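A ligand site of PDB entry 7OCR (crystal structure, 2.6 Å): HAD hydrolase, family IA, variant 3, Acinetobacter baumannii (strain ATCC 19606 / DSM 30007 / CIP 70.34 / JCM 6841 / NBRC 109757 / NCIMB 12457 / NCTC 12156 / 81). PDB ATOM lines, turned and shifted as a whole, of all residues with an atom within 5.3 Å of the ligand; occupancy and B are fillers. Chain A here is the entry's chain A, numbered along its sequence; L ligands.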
ATOM      1  N   GLY A 251     -23.692 -33.510   6.180  1.00  0.00           N
ATOM      2  CA  GLY A 251     -23.328 -32.085   6.027  1.00  0.00           C
ATOM      3  C   GLY A 251     -24.560 -31.195   6.112  1.00  0.00           C
ATOM      4  O   GLY A 251     -25.042 -30.753   5.052  1.00  0.00           O
ATOM      5  N   PHE A 252     -25.045 -30.942   7.336  1.00  0.00           N
ATOM      6  CA  PHE A 252     -26.202 -30.050   7.631  1.00  0.00           C
ATOM      7  C   PHE A 252     -25.782 -28.596   7.385  1.00  0.00           C
ATOM      8  O   PHE A 252     -25.664 -27.820   8.364  1.00  0.00           O
ATOM      9  CB  PHE A 252     -26.703 -30.284   9.057  1.00  0.00           C
ATOM     10  CG  PHE A 252     -27.952 -29.532   9.422  1.00  0.00           C
ATOM     11  CD1 PHE A 252     -29.154 -29.798   8.787  1.00  0.00           C
ATOM     12  CD2 PHE A 252     -27.939 -28.555  10.406  1.00  0.00           C
ATOM     13  CE1 PHE A 252     -30.312 -29.111   9.127  1.00  0.00           C
ATOM     14  CE2 PHE A 252     -29.091 -27.863  10.751  1.00  0.00           C
ATOM     15  CZ  PHE A 252     -30.276 -28.139  10.106  1.00  0.00           C
ATOM     16  N   GLY A 253     -25.551 -28.251   6.119  1.00  0.00           N
ATOM     17  CA  GLY A 253     -25.145 -26.907   5.666  1.00  0.00           C
ATOM     18  C   GLY A 253     -26.274 -26.193   4.950  1.00  0.00           C
ATOM     19  O   GLY A 253     -27.438 -26.616   5.119  1.00  0.00           O
ATOM     20  N   ALA A 254     -25.946 -25.162   4.167  1.00  0.00           N
ATOM     21  CA  ALA A 254     -26.917 -24.316   3.424  1.00  0.00           C
ATOM     22  C   ALA A 254     -27.794 -25.193   2.535  1.00  0.00           C
ATOM     23  O   ALA A 254     -29.033 -25.155   2.707  1.00  0.00           O
ATOM     24  CB  ALA A 254     -26.176 -23.285   2.610  1.00  0.00           C
ATOM     25  N   ILE A 255     -27.181 -25.984   1.649  1.00  0.00           N
ATOM     26  CA  ILE A 255     -27.890 -26.808   0.627  1.00  0.00           C
ATOM     27  C   ILE A 255     -28.482 -28.049   1.301  1.00  0.00           C
ATOM     28  O   ILE A 255     -29.571 -28.493   0.876  1.00  0.00           O
ATOM     29  CB  ILE A 255     -26.954 -27.166  -0.551  1.00  0.00           C
ATOM     30  CG1 ILE A 255     -27.730 -27.402  -1.845  1.00  0.00           C
ATOM     31  CG2 ILE A 255     -26.053 -28.340  -0.199  1.00  0.00           C
ATOM     32  CD1 ILE A 255     -28.414 -26.168  -2.389  1.00  0.00           C
ATOM     33  N   GLY A 256     -27.813 -28.589   2.323  1.00  0.00           N
ATOM     34  CA  GLY A 256     -28.239 -29.790   3.073  1.00  0.00           C
ATOM     35  C   GLY A 256     -29.496 -29.530   3.869  1.00  0.00           C
ATOM     36  O   GLY A 256     -30.459 -30.308   3.724  1.00  0.00           O
ATOM     37  N   SER A 279     -25.586 -34.232   9.989  1.00  0.00           N
ATOM     38  CA  SER A 279     -24.246 -34.139  10.641  1.00  0.00           C
ATOM     39  C   SER A 279     -23.708 -32.707  10.532  1.00  0.00           C
ATOM     40  O   SER A 279     -23.858 -32.097   9.455  1.00  0.00           O
ATOM     41  CB  SER A 279     -23.293 -35.135  10.039  1.00  0.00           C
ATOM     42  OG  SER A 279     -23.005 -34.802   8.686  1.00  0.00           O
ATOM     43  N   THR A 280     -23.109 -32.202  11.616  1.00  0.00           N
ATOM     44  CA  THR A 280     -22.489 -30.840  11.692  1.00  0.00           C
ATOM     45  C   THR A 280     -21.569 -30.767  12.919  1.00  0.00           C
ATOM     46  O   THR A 280     -21.888 -31.397  13.941  1.00  0.00           O
ATOM     47  CB  THR A 280     -23.564 -29.750  11.731  1.00  0.00           C
ATOM     48  OG1 THR A 280     -22.911 -28.484  11.645  1.00  0.00           O
ATOM     49  CG2 THR A 280     -24.432 -29.794  12.971  1.00  0.00           C
ATOM     50  N   ARG A 281     -20.464 -30.022  12.797  1.00  0.00           N
ATOM     51  CA  ARG A 281     -19.496 -29.736  13.887  1.00  0.00           C
ATOM     52  C   ARG A 281     -19.970 -28.516  14.684  1.00  0.00           C
ATOM     53  O   ARG A 281     -19.474 -28.325  15.813  1.00  0.00           O
ATOM     54  CB  ARG A 281     -18.095 -29.498  13.315  1.00  0.00           C
ATOM     55  CG  ARG A 281     -17.553 -30.625  12.454  1.00  0.00           C
ATOM     56  CD  ARG A 281     -16.397 -30.186  11.574  1.00  0.00           C
ATOM     57  NE  ARG A 281     -16.807 -29.208  10.579  1.00  0.00           N
ATOM     58  CZ  ARG A 281     -15.986 -28.525   9.784  1.00  0.00           C
ATOM     59  NH1 ARG A 281     -14.670 -28.709   9.856  1.00  0.00           N
ATOM     60  NH2 ARG A 281     -16.471 -27.649   8.914  1.00  0.00           N
ATOM     61  N   ASN A 282     -20.889 -27.726  14.109  1.00  0.00           N
ATOM     62  CA  ASN A 282     -21.510 -26.538  14.749  1.00  0.00           C
ATOM     63  C   ASN A 282     -22.418 -27.007  15.890  1.00  0.00           C
ATOM     64  O   ASN A 282     -23.542 -27.464  15.617  1.00  0.00           O
ATOM     65  CB  ASN A 282     -22.283 -25.699  13.714  1.00  0.00           C
ATOM     66  CG  ASN A 282     -22.693 -24.339  14.226  1.00  0.00           C
ATOM     67  OD1 ASN A 282     -22.964 -24.159  15.409  1.00  0.00           O
ATOM     68  ND2 ASN A 282     -22.743 -23.362  13.340  1.00  0.00           N
ATOM     69  N   CYS A 335     -23.597 -33.435   1.200  1.00  0.00           N
ATOM     70  CA  CYS A 335     -23.757 -31.970   0.972  1.00  0.00           C
ATOM     71  C   CYS A 335     -22.521 -31.233   1.485  1.00  0.00           C
ATOM     72  O   CYS A 335     -22.679 -30.251   2.238  1.00  0.00           O
ATOM     73  CB  CYS A 335     -25.017 -31.463   1.658  1.00  0.00           C
ATOM     74  SG  CYS A 335     -26.500 -32.431   1.249  1.00  0.00           S
ATOM     75  N   LEU A 336     -21.326 -31.678   1.071  1.00  0.00           N
ATOM     76  CA  LEU A 336     -20.008 -31.133   1.493  1.00  0.00           C
ATOM     77  C   LEU A 336     -19.394 -30.336   0.339  1.00  0.00           C
ATOM     78  O   LEU A 336     -19.720 -30.573  -0.825  1.00  0.00           O
ATOM     79  CB  LEU A 336     -19.094 -32.296   1.877  1.00  0.00           C
ATOM     80  CG  LEU A 336     -19.610 -33.219   2.985  1.00  0.00           C
ATOM     81  CD1 LEU A 336     -18.716 -34.430   3.139  1.00  0.00           C
ATOM     82  CD2 LEU A 336     -19.739 -32.470   4.305  1.00  0.00           C
ATOM     83  N   PRO A 337     -18.486 -29.371   0.627  1.00  0.00           N
ATOM     84  CA  PRO A 337     -17.636 -28.771  -0.404  1.00  0.00           C
ATOM     85  C   PRO A 337     -16.602 -29.778  -0.936  1.00  0.00           C
ATOM     86  O   PRO A 337     -16.487 -30.854  -0.382  1.00  0.00           O
ATOM     87  CB  PRO A 337     -16.926 -27.603   0.297  1.00  0.00           C
ATOM     88  CG  PRO A 337     -17.693 -27.395   1.593  1.00  0.00           C
ATOM     89  CD  PRO A 337     -18.257 -28.756   1.947  1.00  0.00           C
ATOM     90  N   GLU A 338     -15.863 -29.388  -1.976  1.00  0.00           N
ATOM     91  CA  GLU A 338     -14.819 -30.215  -2.639  1.00  0.00           C
ATOM     92  C   GLU A 338     -13.663 -30.471  -1.656  1.00  0.00           C
ATOM     93  O   GLU A 338     -13.062 -31.558  -1.732  1.00  0.00           O
ATOM     94  CB  GLU A 338     -14.314 -29.539  -3.915  1.00  0.00           C
ATOM     95  CG  GLU A 338     -13.457 -30.432  -4.785  1.00  0.00           C
ATOM     96  CD  GLU A 338     -12.869 -29.763  -6.021  1.00  0.00           C
ATOM     97  OE1 GLU A 338     -13.589 -28.977  -6.661  1.00  0.00           O
ATOM     98  OE2 GLU A 338     -11.689 -30.024  -6.324  1.00  0.00           O
ATOM     99  N   GLN A 339     -13.377 -29.509  -0.782  1.00  0.00           N
ATOM    100  CA  GLN A 339     -12.223 -29.521   0.158  1.00  0.00           C
ATOM    101  C   GLN A 339     -12.415 -30.619   1.216  1.00  0.00           C
ATOM    102  O   GLN A 339     -11.409 -31.238   1.606  1.00  0.00           O
ATOM    103  CB  GLN A 339     -12.050 -28.164   0.850  1.00  0.00           C
ATOM    104  CG  GLN A 339     -11.972 -26.986  -0.104  1.00  0.00           C
ATOM    105  CD  GLN A 339     -13.300 -26.280  -0.273  1.00  0.00           C
ATOM    106  OE1 GLN A 339     -13.928 -25.847   0.696  1.00  0.00           O
ATOM    107  NE2 GLN A 339     -13.747 -26.162  -1.514  1.00  0.00           N
ATOM    108  N   ALA A 340     -13.663 -30.859   1.639  1.00  0.00           N
ATOM    109  CA  ALA A 340     -14.033 -31.757   2.765  1.00  0.00           C
ATOM    110  C   ALA A 340     -14.147 -33.207   2.297  1.00  0.00           C
ATOM    111  O   ALA A 340     -14.232 -34.089   3.171  1.00  0.00           O
ATOM    112  CB  ALA A 340     -15.320 -31.272   3.387  1.00  0.00           C
ATOM    113  N   SER A 343     -11.137 -35.593   3.577  1.00  0.00           N
ATOM    114  CA  SER A 343     -11.138 -35.820   5.053  1.00  0.00           C
ATOM    115  C   SER A 343     -12.350 -36.664   5.472  1.00  0.00           C
ATOM    116  O   SER A 343     -12.175 -37.552   6.325  1.00  0.00           O
ATOM    117  CB  SER A 343     -11.097 -34.505   5.793  1.00  0.00           C
ATOM    118  OG  SER A 343     -12.201 -33.679   5.436  1.00  0.00           O
ATOM    119  N   GLU A 344     -13.530 -36.384   4.897  1.00  0.00           N
ATOM    120  CA  GLU A 344     -14.821 -37.015   5.290  1.00  0.00           C
ATOM    121  C   GLU A 344     -14.967 -38.419   4.681  1.00  0.00           C
ATOM    122  O   GLU A 344     -15.826 -39.175   5.172  1.00  0.00           O
ATOM    123  CB  GLU A 344     -16.003 -36.122   4.873  1.00  0.00           C
ATOM    124  CG  GLU A 344     -16.095 -34.837   5.667  1.00  0.00           C
ATOM    125  CD  GLU A 344     -16.533 -34.987   7.113  1.00  0.00           C
ATOM    126  OE1 GLU A 344     -17.450 -35.784   7.375  1.00  0.00           O
ATOM    127  OE2 GLU A 344     -15.941 -34.315   7.977  1.00  0.00           O
ATOM    128  N   ILE A 372     -24.294 -34.096  -3.812  1.00  0.00           N
ATOM    129  CA  ILE A 372     -24.616 -32.648  -3.959  1.00  0.00           C
ATOM    130  C   ILE A 372     -23.301 -31.865  -3.978  1.00  0.00           C
ATOM    131  O   ILE A 372     -22.709 -31.679  -2.895  1.00  0.00           O
ATOM    132  CB  ILE A 372     -25.574 -32.158  -2.851  1.00  0.00           C
ATOM    133  CG1 ILE A 372     -26.722 -33.139  -2.587  1.00  0.00           C
ATOM    134  CG2 ILE A 372     -26.077 -30.758  -3.151  1.00  0.00           C
ATOM    135  CD1 ILE A 372     -27.537 -33.481  -3.824  1.00  0.00           C
ATOM    136  N   LEU A 373     -22.843 -31.454  -5.158  1.00  0.00           N
ATOM    137  CA  LEU A 373     -21.549 -30.747  -5.372  1.00  0.00           C
ATOM    138  C   LEU A 373     -21.572 -30.060  -6.747  1.00  0.00           C
ATOM    139  O   LEU A 373     -21.795 -30.767  -7.749  1.00  0.00           O
ATOM    140  CB  LEU A 373     -20.417 -31.779  -5.266  1.00  0.00           C
ATOM    141  CG  LEU A 373     -19.008 -31.251  -5.508  1.00  0.00           C
ATOM    142  CD1 LEU A 373     -18.715 -30.010  -4.670  1.00  0.00           C
ATOM    143  CD2 LEU A 373     -17.971 -32.325  -5.215  1.00  0.00           C
ATOM    144  N   ASN A 374     -21.329 -28.752  -6.774  1.00  0.00           N
ATOM    145  CA  ASN A 374     -21.366 -27.895  -7.997  1.00  0.00           C
ATOM    146  C   ASN A 374     -20.006 -27.985  -8.701  1.00  0.00           C
ATOM    147  O   ASN A 374     -19.331 -26.942  -8.819  1.00  0.00           O
ATOM    148  CB  ASN A 374     -21.762 -26.458  -7.665  1.00  0.00           C
ATOM    149  CG  ASN A 374     -22.146 -25.634  -8.870  1.00  0.00           C
ATOM    150  OD1 ASN A 374     -21.929 -26.041 -10.013  1.00  0.00           O
ATOM    151  ND2 ASN A 374     -22.726 -24.468  -8.642  1.00  0.00           N
ATOM    152  N   VAL A 414     -28.155 -29.231  -8.819  1.00  0.00           N
ATOM    153  CA  VAL A 414     -29.008 -28.361  -7.946  1.00  0.00           C
ATOM    154  C   VAL A 414     -28.917 -26.922  -8.454  1.00  0.00           C
ATOM    155  O   VAL A 414     -27.797 -26.491  -8.805  1.00  0.00           O
ATOM    156  CB  VAL A 414     -28.584 -28.470  -6.472  1.00  0.00           C
ATOM    157  CG1 VAL A 414     -29.361 -27.505  -5.590  1.00  0.00           C
ATOM    158  CG2 VAL A 414     -28.705 -29.896  -5.958  1.00  0.00           C
ATOM    159  N   ARG A 416     -30.996 -24.315  -6.767  1.00  0.00           N
ATOM    160  CA  ARG A 416     -31.451 -23.446  -5.646  1.00  0.00           C
ATOM    161  C   ARG A 416     -30.235 -22.847  -4.933  1.00  0.00           C
ATOM    162  O   ARG A 416     -29.401 -23.628  -4.442  1.00  0.00           O
ATOM    163  CB  ARG A 416     -32.316 -24.221  -4.654  1.00  0.00           C
ATOM    164  CG  ARG A 416     -32.854 -23.362  -3.510  1.00  0.00           C
ATOM    165  CD  ARG A 416     -33.709 -24.128  -2.522  1.00  0.00           C
ATOM    166  NE  ARG A 416     -35.043 -24.425  -3.036  1.00  0.00           N
ATOM    167  CZ  ARG A 416     -36.047 -24.892  -2.316  1.00  0.00           C
ATOM    168  NH1 ARG A 416     -35.902 -25.139  -1.021  1.00  0.00           N
ATOM    169  NH2 ARG A 416     -37.222 -25.123  -2.882  1.00  0.00           N
ATOM    170  N   MET A 417     -30.146 -21.507  -4.891  1.00  0.00           N
ATOM    171  CA  MET A 417     -29.155 -20.752  -4.076  1.00  0.00           C
ATOM    172  C   MET A 417     -29.683 -20.658  -2.635  1.00  0.00           C
ATOM    173  O   MET A 417     -30.856 -20.261  -2.470  1.00  0.00           O
ATOM    174  CB  MET A 417     -28.926 -19.348  -4.627  1.00  0.00           C
ATOM    175  CG  MET A 417     -28.108 -19.321  -5.903  1.00  0.00           C
ATOM    176  SD  MET A 417     -27.656 -17.634  -6.399  1.00  0.00           S
ATOM    177  CE  MET A 417     -26.545 -17.971  -7.765  1.00  0.00           C
ATOM    178  N   VAL A 418     -28.852 -21.008  -1.650  1.00  0.00           N
ATOM    179  CA  VAL A 418     -29.206 -20.987  -0.196  1.00  0.00           C
ATOM    180  C   VAL A 418     -28.030 -20.400   0.588  1.00  0.00           C
ATOM    181  O   VAL A 418     -26.871 -20.620   0.180  1.00  0.00           O
ATOM    182  CB  VAL A 418     -29.571 -22.391   0.316  1.00  0.00           C
ATOM    183  CG1 VAL A 418     -30.092 -22.331   1.746  1.00  0.00           C
ATOM    184  CG2 VAL A 418     -30.564 -23.088  -0.590  1.00  0.00           C
ATOM    185  N   LYS A 420     -26.718 -20.150   4.771  1.00  0.00           N
ATOM    186  CA  LYS A 420     -26.854 -20.579   6.199  1.00  0.00           C
ATOM    187  C   LYS A 420     -26.727 -19.344   7.086  1.00  0.00           C
ATOM    188  O   LYS A 420     -25.952 -18.427   6.728  1.00  0.00           O
ATOM    189  CB  LYS A 420     -25.797 -21.638   6.550  1.00  0.00           C
ATOM    190  CG  LYS A 420     -25.991 -22.293   7.914  1.00  0.00           C
ATOM    191  CD  LYS A 420     -25.090 -23.488   8.145  1.00  0.00           C
ATOM    192  CE  LYS A 420     -23.633 -23.115   8.348  1.00  0.00           C
ATOM    193  NZ  LYS A 420     -22.802 -24.308   8.610  1.00  0.00           N
ATOM    194  N   LYS A 527     -26.523 -26.305 -16.846  1.00  0.00           N
ATOM    195  CA  LYS A 527     -26.080 -25.724 -15.552  1.00  0.00           C
ATOM    196  C   LYS A 527     -24.779 -24.944 -15.759  1.00  0.00           C
ATOM    197  O   LYS A 527     -24.640 -23.844 -15.190  1.00  0.00           O
ATOM    198  CB  LYS A 527     -25.901 -26.835 -14.511  1.00  0.00           C
ATOM    199  CG  LYS A 527     -25.367 -26.389 -13.156  1.00  0.00           C
ATOM    200  CD  LYS A 527     -26.353 -25.598 -12.339  1.00  0.00           C
ATOM    201  CE  LYS A 527     -25.744 -24.984 -11.106  1.00  0.00           C
ATOM    202  NZ  LYS A 527     -26.753 -24.281 -10.275  1.00  0.00           N
HETATM  203  P1  LIG L   1     -21.444 -25.023   3.720  1.00  0.00           P
HETATM  204  O1  LIG L   1     -20.009 -24.686   3.957  1.00  0.00           O
HETATM  205  O2  LIG L   1     -22.500 -23.978   3.895  1.00  0.00           O
HETATM  206  O3  LIG L   1     -21.837 -26.351   4.625  1.00  0.00           O
HETATM  207  C1  LIG L   1     -21.096 -27.409   4.079  1.00  0.00           C
HETATM  208  C2  LIG L   1     -21.107 -28.632   4.995  1.00  0.00           C
HETATM  209  O4  LIG L   1     -19.855 -29.297   4.857  1.00  0.00           O
HETATM  210  C3  LIG L   1     -21.325 -28.244   6.482  1.00  0.00           C
HETATM  211  O5  LIG L   1     -22.064 -29.250   7.114  1.00  0.00           O
HETATM  212  C4  LIG L   1     -19.888 -28.220   7.042  1.00  0.00           C
HETATM  213  O6  LIG L   1     -19.791 -28.659   8.302  1.00  0.00           O
HETATM  214  C5  LIG L   1     -19.160 -29.255   6.103  1.00  0.00           C
HETATM  215  N1  LIG L   1     -17.770 -28.837   5.812  1.00  0.00           N
HETATM  216  C6  LIG L   1     -17.336 -27.712   5.081  1.00  0.00           C
HETATM  217  N2  LIG L   1     -15.984 -27.611   5.004  1.00  0.00           N
HETATM  218  C7  LIG L   1     -15.531 -28.725   5.725  1.00  0.00           C
HETATM  219  C8  LIG L   1     -14.234 -29.195   6.008  1.00  0.00           C
HETATM  220  N3  LIG L   1     -13.131 -28.502   5.548  1.00  0.00           N
HETATM  221  N4  LIG L   1     -14.014 -30.334   6.747  1.00  0.00           N
HETATM  222  C9  LIG L   1     -15.168 -30.977   7.174  1.00  0.00           C
HETATM  223  N5  LIG L   1     -16.469 -30.665   6.987  1.00  0.00           N
HETATM  224  C10 LIG L   1     -16.636 -29.504   6.230  1.00  0.00           C
HETATM  225  O7  LIG L   1     -21.377 -25.434   2.111  1.00  0.00           O
HETATM  226  P2  LIG L   1     -22.849 -25.364   1.485  1.00  0.00           P
HETATM  227  O8  LIG L   1     -23.724 -26.336   2.181  1.00  0.00           O
HETATM  228  O9  LIG L   1     -23.292 -23.962   1.140  1.00  0.00           O
HETATM  229  O10 LIG L   1     -22.789 -26.079  -0.142  1.00  0.00           O
HETATM  230  C11 LIG L   1     -22.258 -27.347  -0.065  1.00  0.00           C
HETATM  231  C12 LIG L   1     -22.092 -27.881  -1.469  1.00  0.00           C
HETATM  232  O11 LIG L   1     -23.323 -27.707  -2.204  1.00  0.00           O
HETATM  233  C13 LIG L   1     -20.996 -27.044  -2.204  1.00  0.00           C
HETATM  234  O12 LIG L   1     -20.138 -27.907  -2.858  1.00  0.00           O
HETATM  235  C14 LIG L   1     -21.805 -26.200  -3.194  1.00  0.00           C
HETATM  236  O13 LIG L   1     -21.152 -25.975  -4.398  1.00  0.00           O
HETATM  237  C15 LIG L   1     -23.017 -27.132  -3.456  1.00  0.00           C
HETATM  238  N6  LIG L   1     -24.182 -26.354  -3.945  1.00  0.00           N
HETATM  239  C16 LIG L   1     -24.769 -25.402  -3.123  1.00  0.00           C
HETATM  240  C17 LIG L   1     -25.553 -24.422  -3.678  1.00  0.00           C
HETATM  241  C18 LIG L   1     -25.598 -23.159  -2.944  1.00  0.00           C
HETATM  242  O14 LIG L   1     -25.313 -22.060  -3.433  1.00  0.00           O
HETATM  243  N7  LIG L   1     -25.992 -23.195  -1.618  1.00  0.00           N
HETATM  244  C19 LIG L   1     -26.072 -24.525  -5.075  1.00  0.00           C
HETATM  245  C20 LIG L   1     -25.379 -25.588  -5.845  1.00  0.00           C
HETATM  246  C21 LIG L   1     -24.695 -26.566  -5.236  1.00  0.00           C
HETATM  247  P3  LIG L   1     -20.422 -27.471   9.573  1.00  0.00           P
HETATM  248  O15 LIG L   1     -21.888 -27.686   9.314  1.00  0.00           O
HETATM  249  O16 LIG L   1     -19.851 -28.020  10.874  1.00  0.00           O
HETATM  250  O17 LIG L   1     -19.815 -26.210   9.026  1.00  0.00           O
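The backbone NH (N) of Phe 252 sits at hydrogen-bond distance from an oxygen (O5) of the ligand (3.4 Å). O of Leu 336 lies within hydrogen-bond range of O12 of the ligand (3.4 Å). An oxygen (O8) of the ligand lies within hydrogen-bond range of the backbone NH (N) of Ala 254, at 3.2 Å. An oxygen (O17) of the ligand lies within salt-bridge range of the side-chain amino group (NZ) of Lys 420 (3.6 Å). An oxygen (O16) of the ligand lies within hydrogen-bond range of the backbone NH (N) of Arg 281. OG1 of Thr 280 lies within hydrogen-bond range of O15 of the ligand, 2.7 Å away. N of Asn 282 lies within hydrogen-bond range of O16 of the ligand (3.4 Å). An oxygen (O16) of the ligand lies within salt-bridge range of the guanidinium group (NE) of Arg 281 (3.3 Å). The backbone carbonyl oxygen of Val 418 lies within hydrogen-bond range of a nitrogen (N7) of the ligand (3.3 Å).
The backbone carbonyl oxygen of Ala 340 lies within hydrogen-bond range of the side-chain hydroxyl of Ser 343, at 3.1 Å. OG1 of Thr 280 sits at hydrogen-bond distance from N of Asn 282 (3.3 Å). N of Phe 252 lies within hydrogen-bond range of O of Ser 279 (2.7 Å). O of Val 414 sits at hydrogen-bond distance from NZ of Lys 527 (2.9 Å). The backbone NH (N) of Gly 251 lies within hydrogen-bond range of the side-chain hydroxyl (OG) of Ser 279 (2.9 Å).
Merely in contact with the ligand: Gly 251 (3.3 Å), Gly 253 (3.5 Å), Ile 255 (3.4 Å), Cys 335 (3.6 Å), Pro 337 (3.4 Å), Ala 340 (3.5 Å), Glu 344 (3.5 Å), Leu 373 (3.1 Å), Asn 374 (3.4 Å), Val 414 (3.9 Å) and Arg 416 (3.5 Å).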
